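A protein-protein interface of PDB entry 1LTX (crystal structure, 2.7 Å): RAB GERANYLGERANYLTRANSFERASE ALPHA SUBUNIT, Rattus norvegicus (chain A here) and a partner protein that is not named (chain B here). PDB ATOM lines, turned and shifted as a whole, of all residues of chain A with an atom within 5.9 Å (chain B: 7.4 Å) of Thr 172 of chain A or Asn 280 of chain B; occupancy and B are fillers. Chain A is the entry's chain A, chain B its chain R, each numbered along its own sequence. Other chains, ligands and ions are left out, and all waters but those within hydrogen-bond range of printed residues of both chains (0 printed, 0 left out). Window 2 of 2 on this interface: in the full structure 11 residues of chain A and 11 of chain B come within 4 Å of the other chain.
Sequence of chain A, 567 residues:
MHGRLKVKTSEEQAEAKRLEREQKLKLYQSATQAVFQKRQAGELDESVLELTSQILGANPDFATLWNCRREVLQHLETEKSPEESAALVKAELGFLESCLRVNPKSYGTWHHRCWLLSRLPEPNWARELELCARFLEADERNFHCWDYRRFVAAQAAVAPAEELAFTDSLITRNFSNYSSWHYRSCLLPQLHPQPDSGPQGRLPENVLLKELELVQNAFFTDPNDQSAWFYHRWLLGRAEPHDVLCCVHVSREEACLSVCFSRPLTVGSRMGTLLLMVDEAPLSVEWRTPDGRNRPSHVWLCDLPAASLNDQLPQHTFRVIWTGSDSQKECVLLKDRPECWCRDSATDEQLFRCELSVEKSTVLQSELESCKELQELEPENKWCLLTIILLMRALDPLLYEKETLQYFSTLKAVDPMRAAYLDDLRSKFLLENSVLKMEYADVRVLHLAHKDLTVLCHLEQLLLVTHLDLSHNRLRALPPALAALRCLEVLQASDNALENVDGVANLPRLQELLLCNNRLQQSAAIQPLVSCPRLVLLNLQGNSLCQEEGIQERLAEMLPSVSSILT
The backbone carbonyl oxygen (O) of Phe 279 of chain B sits close to the side-chain amide oxygen (OD1) of Asn 217 of chain A (3.4 Å).
The side-chain amide oxygen (OD1) of Asn 217 of chain A sits at hydrogen-bond distance from the side-chain amino group (NZ) of Lys 289 of chain B (3.4 Å).
OG1 of Thr 172 of chain A is in hydrogen-bond range of O of Ser 169 of chain A (2.8 Å).
O of Ile 171 of chain A lies close to ND2 of Asn 177 of chain A (3.3 Å).
ND2 of Asn 217 of chain A lies within hydrogen-bond range of O of Leu 214 of chain A.
The backbone carbonyl oxygen of Ala 276 of chain B lies within hydrogen-bond range of the side-chain amide nitrogen of Asn 280 of chain B (2.9 Å).
O of Phe 279 of chain B sits at hydrogen-bond distance from NZ of Lys 289 of chain B, at 3.0 Å.
The backbone carbonyl oxygen (O) of Ser 281 of chain B sits at hydrogen-bond distance from the side-chain amino group (NZ) of Lys 289 of chain B (2.9 Å).
CZ of Phe 279 of chain B touches CG2 of Ile 171 of chain A, at 3.8 Å.
Thr 172 of chain A touches Ala 276 of chain B.
Thr 172 of chain A touches Phe 279 of chain B (CG2 to CE2, 3.3 Å).
Thr 172 of chain A touches Asn 280 of chain B.
Phe 279 of chain B touches Leu 214 of chain A (CZ to CD1, 3.7 Å).
Of chain B, only Ala 276 (3.5 Å), Phe 279 (3.3 Å) and Asn 280 (3.4 Å) come within 4 Å of Thr 172 of chain A.
Of the printed residues of chain B, Ile 171 of chain A touches Phe 279.
Printed residues of chain A within 4 Å of Lys 289 of chain B: Asn 217 (3.4 Å).
Of the printed residues of chain B, Leu 214 of chain A touches Phe 279 (3.7 Å).
Of the printed residues of chain A, Phe 279 of chain B touches Ile 171 (3.8 Å), Thr 172 (3.3 Å), Leu 214 (3.7 Å) and Asn 217 (3.4 Å).
Of the printed residues of chain A, Ala 276 of chain B touches Thr 172.
The nearest printed residue of chain B that does not touch Asn 217 of chain A is Asn 280 of chain B (5.3 Å).
Of the 11 printed residues of chain A, 4 touch a printed residue of chain B.
Printed residues of chain A that touch a printed residue of chain B: Ile 171, Thr 172, Leu 214 and Asn 217.
Of the 11 printed residues of chain B, 4 touch a printed residue of chain A.
Hydrophobic or aromatic side chains of chain B within 4 Å of the printed part of chain A: Ala 276 and Phe 279.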
ATOM      1  N   THR A 167      23.028 -13.816  -8.960  1.00  0.00           N
ATOM      2  CA  THR A 167      24.176 -13.088  -8.423  1.00  0.00           C
ATOM      3  C   THR A 167      24.192 -13.090  -6.905  1.00  0.00           C
ATOM      4  O   THR A 167      25.263 -13.209  -6.300  1.00  0.00           O
ATOM      5  CB  THR A 167      24.239 -11.624  -8.925  1.00  0.00           C
ATOM      6  OG1 THR A 167      23.106 -10.887  -8.456  1.00  0.00           O
ATOM      7  CG2 THR A 167      24.272 -11.593 -10.428  1.00  0.00           C
ATOM      8  N   ASP A 168      23.015 -12.966  -6.286  1.00  0.00           N
ATOM      9  CA  ASP A 168      22.942 -12.977  -4.829  1.00  0.00           C
ATOM     10  C   ASP A 168      23.493 -14.301  -4.299  1.00  0.00           C
ATOM     11  O   ASP A 168      24.044 -14.358  -3.196  1.00  0.00           O
ATOM     12  CB  ASP A 168      21.505 -12.799  -4.337  1.00  0.00           C
ATOM     13  CG  ASP A 168      21.444 -12.422  -2.853  1.00  0.00           C
ATOM     14  OD1 ASP A 168      21.995 -13.172  -2.008  1.00  0.00           O
ATOM     15  OD2 ASP A 168      20.847 -11.367  -2.536  1.00  0.00           O
ATOM     16  N   SER A 169      23.348 -15.361  -5.090  1.00  0.00           N
ATOM     17  CA  SER A 169      23.853 -16.664  -4.687  1.00  0.00           C
ATOM     18  C   SER A 169      25.356 -16.783  -4.965  1.00  0.00           C
ATOM     19  O   SER A 169      26.115 -17.211  -4.096  1.00  0.00           O
ATOM     20  CB  SER A 169      23.077 -17.778  -5.395  1.00  0.00           C
ATOM     21  OG  SER A 169      23.198 -17.685  -6.797  1.00  0.00           O
ATOM     22  N   LEU A 170      25.792 -16.402  -6.163  1.00  0.00           N
ATOM     23  CA  LEU A 170      27.217 -16.459  -6.498  1.00  0.00           C
ATOM     24  C   LEU A 170      28.045 -15.583  -5.550  1.00  0.00           C
ATOM     25  O   LEU A 170      29.252 -15.778  -5.400  1.00  0.00           O
ATOM     26  CB  LEU A 170      27.453 -15.994  -7.941  1.00  0.00           C
ATOM     27  CG  LEU A 170      27.452 -17.065  -9.029  1.00  0.00           C
ATOM     28  CD1 LEU A 170      28.607 -18.024  -8.802  1.00  0.00           C
ATOM     29  CD2 LEU A 170      26.133 -17.808  -9.002  1.00  0.00           C
ATOM     30  N   ILE A 171      27.385 -14.619  -4.917  1.00  0.00           N
ATOM     31  CA  ILE A 171      28.046 -13.707  -3.998  1.00  0.00           C
ATOM     32  C   ILE A 171      28.217 -14.265  -2.592  1.00  0.00           C
ATOM     33  O   ILE A 171      29.257 -14.064  -1.961  1.00  0.00           O
ATOM     34  CB  ILE A 171      27.285 -12.368  -3.936  1.00  0.00           C
ATOM     35  CG1 ILE A 171      27.696 -11.513  -5.137  1.00  0.00           C
ATOM     36  CG2 ILE A 171      27.551 -11.662  -2.616  1.00  0.00           C
ATOM     37  CD1 ILE A 171      26.964 -10.205  -5.270  1.00  0.00           C
ATOM     38  N   THR A 172      27.193 -14.956  -2.103  1.00  0.00           N
ATOM     39  CA  THR A 172      27.215 -15.551  -0.765  1.00  0.00           C
ATOM     40  C   THR A 172      28.310 -16.624  -0.614  1.00  0.00           C
ATOM     41  O   THR A 172      29.032 -16.643   0.381  1.00  0.00           O
ATOM     42  CB  THR A 172      25.848 -16.185  -0.441  1.00  0.00           C
ATOM     43  OG1 THR A 172      25.588 -17.242  -1.368  1.00  0.00           O
ATOM     44  CG2 THR A 172      24.731 -15.154  -0.568  1.00  0.00           C
ATOM     45  N   ARG A 173      28.432 -17.493  -1.619  1.00  0.00           N
ATOM     46  CA  ARG A 173      29.411 -18.590  -1.624  1.00  0.00           C
ATOM     47  C   ARG A 173      30.846 -18.138  -1.920  1.00  0.00           C
ATOM     48  O   ARG A 173      31.800 -18.597  -1.286  1.00  0.00           O
ATOM     49  CB  ARG A 173      29.020 -19.656  -2.671  1.00  0.00           C
ATOM     50  CG  ARG A 173      27.512 -19.895  -2.806  1.00  0.00           C
ATOM     51  CD  ARG A 173      27.183 -21.256  -3.421  1.00  0.00           C
ATOM     52  NE  ARG A 173      27.588 -21.398  -4.820  1.00  0.00           N
ATOM     53  CZ  ARG A 173      26.830 -21.068  -5.864  1.00  0.00           C
ATOM     54  NH1 ARG A 173      25.611 -20.568  -5.674  1.00  0.00           N
ATOM     55  NH2 ARG A 173      27.285 -21.249  -7.103  1.00  0.00           N
ATOM     56  N   ASN A 174      30.989 -17.252  -2.900  1.00  0.00           N
ATOM     57  CA  ASN A 174      32.300 -16.748  -3.313  1.00  0.00           C
ATOM     58  C   ASN A 174      32.905 -15.663  -2.409  1.00  0.00           C
ATOM     59  O   ASN A 174      32.190 -14.940  -1.698  1.00  0.00           O
ATOM     60  CB  ASN A 174      32.212 -16.253  -4.759  1.00  0.00           C
ATOM     61  CG  ASN A 174      32.112 -17.395  -5.752  1.00  0.00           C
ATOM     62  OD1 ASN A 174      31.511 -17.265  -6.819  1.00  0.00           O
ATOM     63  ND2 ASN A 174      32.720 -18.525  -5.409  1.00  0.00           N
ATOM     64  N   ASN A 177      34.237 -11.942  -5.888  1.00  0.00           N
ATOM     65  CA  ASN A 177      33.346 -11.898  -7.039  1.00  0.00           C
ATOM     66  C   ASN A 177      33.077 -10.459  -7.456  1.00  0.00           C
ATOM     67  O   ASN A 177      32.174  -9.802  -6.940  1.00  0.00           O
ATOM     68  CB  ASN A 177      32.022 -12.600  -6.706  1.00  0.00           C
ATOM     69  CG  ASN A 177      31.639 -12.462  -5.226  1.00  0.00           C
ATOM     70  OD1 ASN A 177      31.933 -11.447  -4.576  1.00  0.00           O
ATOM     71  ND2 ASN A 177      30.970 -13.485  -4.692  1.00  0.00           N
ATOM     72  N   LEU A 214      23.153  -5.660   1.826  1.00  0.00           N
ATOM     73  CA  LEU A 214      23.698  -6.827   1.156  1.00  0.00           C
ATOM     74  C   LEU A 214      25.215  -6.669   0.984  1.00  0.00           C
ATOM     75  O   LEU A 214      25.955  -7.655   0.948  1.00  0.00           O
ATOM     76  CB  LEU A 214      23.035  -7.016  -0.217  1.00  0.00           C
ATOM     77  CG  LEU A 214      23.520  -8.227  -1.027  1.00  0.00           C
ATOM     78  CD1 LEU A 214      23.184  -9.508  -0.273  1.00  0.00           C
ATOM     79  CD2 LEU A 214      22.874  -8.244  -2.400  1.00  0.00           C
ATOM     80  N   ASN A 217      27.703  -6.532   4.644  1.00  0.00           N
ATOM     81  CA  ASN A 217      28.239  -7.759   5.211  1.00  0.00           C
ATOM     82  C   ASN A 217      29.116  -8.493   4.215  1.00  0.00           C
ATOM     83  O   ASN A 217      29.855  -9.403   4.576  1.00  0.00           O
ATOM     84  CB  ASN A 217      27.112  -8.673   5.726  1.00  0.00           C
ATOM     85  CG  ASN A 217      26.207  -9.190   4.623  1.00  0.00           C
ATOM     86  OD1 ASN A 217      25.248  -9.917   4.890  1.00  0.00           O
ATOM     87  ND2 ASN A 217      26.505  -8.821   3.381  1.00  0.00           N
ATOM     88  N   SER B 274      30.205 -22.016   7.791  1.00  0.00           N
ATOM     89  CA  SER B 274      30.813 -21.836   6.477  1.00  0.00           C
ATOM     90  C   SER B 274      30.745 -20.360   6.108  1.00  0.00           C
ATOM     91  O   SER B 274      29.952 -19.601   6.688  1.00  0.00           O
ATOM     92  CB  SER B 274      30.055 -22.632   5.426  1.00  0.00           C
ATOM     93  OG  SER B 274      28.808 -22.009   5.171  1.00  0.00           O
ATOM     94  N   ARG B 275      31.571 -19.960   5.139  1.00  0.00           N
ATOM     95  CA  ARG B 275      31.602 -18.577   4.663  1.00  0.00           C
ATOM     96  C   ARG B 275      30.193 -18.168   4.218  1.00  0.00           C
ATOM     97  O   ARG B 275      29.694 -17.095   4.582  1.00  0.00           O
ATOM     98  CB  ARG B 275      32.598 -18.449   3.501  1.00  0.00           C
ATOM     99  CG  ARG B 275      34.103 -18.513   3.912  1.00  0.00           C
ATOM    100  CD  ARG B 275      34.551 -19.865   4.558  1.00  0.00           C
ATOM    101  NE  ARG B 275      35.928 -19.849   5.100  1.00  0.00           N
ATOM    102  CZ  ARG B 275      37.049 -19.905   4.372  1.00  0.00           C
ATOM    103  NH1 ARG B 275      36.988 -19.985   3.043  1.00  0.00           N
ATOM    104  NH2 ARG B 275      38.238 -19.883   4.973  1.00  0.00           N
ATOM    105  N   ALA B 276      29.547 -19.045   3.455  1.00  0.00           N
ATOM    106  CA  ALA B 276      28.198 -18.797   2.978  1.00  0.00           C
ATOM    107  C   ALA B 276      27.205 -18.658   4.125  1.00  0.00           C
ATOM    108  O   ALA B 276      26.301 -17.830   4.063  1.00  0.00           O
ATOM    109  CB  ALA B 276      27.771 -19.912   2.060  1.00  0.00           C
ATOM    110  N   ASP B 277      27.366 -19.465   5.175  1.00  0.00           N
ATOM    111  CA  ASP B 277      26.455 -19.405   6.321  1.00  0.00           C
ATOM    112  C   ASP B 277      26.547 -18.080   7.041  1.00  0.00           C
ATOM    113  O   ASP B 277      25.527 -17.446   7.307  1.00  0.00           O
ATOM    114  CB  ASP B 277      26.751 -20.500   7.346  1.00  0.00           C
ATOM    115  CG  ASP B 277      26.526 -21.889   6.805  1.00  0.00           C
ATOM    116  OD1 ASP B 277      25.550 -22.095   6.040  1.00  0.00           O
ATOM    117  OD2 ASP B 277      27.328 -22.782   7.166  1.00  0.00           O
ATOM    118  N   VAL B 278      27.775 -17.683   7.376  1.00  0.00           N
ATOM    119  CA  VAL B 278      28.013 -16.428   8.079  1.00  0.00           C
ATOM    120  C   VAL B 278      27.357 -15.277   7.336  1.00  0.00           C
ATOM    121  O   VAL B 278      26.685 -14.432   7.939  1.00  0.00           O
ATOM    122  CB  VAL B 278      29.503 -16.128   8.187  1.00  0.00           C
ATOM    123  CG1 VAL B 278      29.714 -14.911   9.064  1.00  0.00           C
ATOM    124  CG2 VAL B 278      30.230 -17.332   8.736  1.00  0.00           C
ATOM    125  N   PHE B 279      27.563 -15.252   6.020  1.00  0.00           N
ATOM    126  CA  PHE B 279      26.988 -14.225   5.162  1.00  0.00           C
ATOM    127  C   PHE B 279      25.469 -14.159   5.359  1.00  0.00           C
ATOM    128  O   PHE B 279      24.954 -13.184   5.901  1.00  0.00           O
ATOM    129  CB  PHE B 279      27.312 -14.535   3.698  1.00  0.00           C
ATOM    130  CG  PHE B 279      26.872 -13.467   2.730  1.00  0.00           C
ATOM    131  CD1 PHE B 279      27.770 -12.496   2.284  1.00  0.00           C
ATOM    132  CD2 PHE B 279      25.560 -13.439   2.249  1.00  0.00           C
ATOM    133  CE1 PHE B 279      27.372 -11.514   1.369  1.00  0.00           C
ATOM    134  CE2 PHE B 279      25.148 -12.461   1.335  1.00  0.00           C
ATOM    135  CZ  PHE B 279      26.057 -11.498   0.895  1.00  0.00           C
ATOM    136  N   ASN B 280      24.758 -15.207   4.949  1.00  0.00           N
ATOM    137  CA  ASN B 280      23.301 -15.223   5.073  1.00  0.00           C
ATOM    138  C   ASN B 280      22.750 -15.058   6.485  1.00  0.00           C
ATOM    139  O   ASN B 280      21.658 -14.518   6.666  1.00  0.00           O
ATOM    140  CB  ASN B 280      22.727 -16.504   4.473  1.00  0.00           C
ATOM    141  CG  ASN B 280      23.013 -16.632   2.993  1.00  0.00           C
ATOM    142  OD1 ASN B 280      22.142 -17.024   2.215  1.00  0.00           O
ATOM    143  ND2 ASN B 280      24.243 -16.314   2.595  1.00  0.00           N
ATOM    144  N   SER B 281      23.492 -15.536   7.480  1.00  0.00           N
ATOM    145  CA  SER B 281      23.054 -15.439   8.872  1.00  0.00           C
ATOM    146  C   SER B 281      22.508 -14.056   9.167  1.00  0.00           C
ATOM    147  O   SER B 281      23.090 -13.055   8.761  1.00  0.00           O
ATOM    148  CB  SER B 281      24.214 -15.731   9.828  1.00  0.00           C
ATOM    149  OG  SER B 281      23.840 -15.454  11.167  1.00  0.00           O
ATOM    150  N   LYS B 282      21.385 -13.999   9.867  1.00  0.00           N
ATOM    151  CA  LYS B 282      20.781 -12.723  10.212  1.00  0.00           C
ATOM    152  C   LYS B 282      20.700 -12.667  11.726  1.00  0.00           C
ATOM    153  O   LYS B 282      19.841 -11.991  12.291  1.00  0.00           O
ATOM    154  CB  LYS B 282      19.380 -12.626   9.611  1.00  0.00           C
ATOM    155  CG  LYS B 282      19.251 -13.324   8.271  1.00  0.00           C
ATOM    156  CD  LYS B 282      17.951 -12.950   7.580  1.00  0.00           C
ATOM    157  CE  LYS B 282      18.072 -11.618   6.834  1.00  0.00           C
ATOM    158  NZ  LYS B 282      19.004 -11.706   5.662  1.00  0.00           N
ATOM    159  N   GLN B 283      21.612 -13.385  12.373  1.00  0.00           N
ATOM    160  CA  GLN B 283      21.652 -13.463  13.829  1.00  0.00           C
ATOM    161  C   GLN B 283      22.972 -12.945  14.380  1.00  0.00           C
ATOM    162  O   GLN B 283      23.042 -12.454  15.510  1.00  0.00           O
ATOM    163  CB  GLN B 283      21.451 -14.914  14.266  1.00  0.00           C
ATOM    164  CG  GLN B 283      20.153 -15.539  13.768  1.00  0.00           C
ATOM    165  CD  GLN B 283      18.927 -14.933  14.430  1.00  0.00           C
ATOM    166  OE1 GLN B 283      18.798 -14.946  15.658  1.00  0.00           O
ATOM    167  NE2 GLN B 283      18.017 -14.397  13.620  1.00  0.00           N
ATOM    168  N   LYS B 289      30.161 -11.470  12.526  1.00  0.00           N
ATOM    169  CA  LYS B 289      30.502 -12.104  11.263  1.00  0.00           C
ATOM    170  C   LYS B 289      31.981 -11.942  10.948  1.00  0.00           C
ATOM    171  O   LYS B 289      32.593 -12.793  10.300  1.00  0.00           O
ATOM    172  CB  LYS B 289      29.674 -11.508  10.137  1.00  0.00           C
ATOM    173  CG  LYS B 289      28.193 -11.495  10.419  1.00  0.00           C
ATOM    174  CD  LYS B 289      27.426 -11.234   9.135  1.00  0.00           C
ATOM    175  CE  LYS B 289      25.929 -11.202   9.367  1.00  0.00           C
ATOM    176  NZ  LYS B 289      25.208 -11.188   8.069  1.00  0.00           N
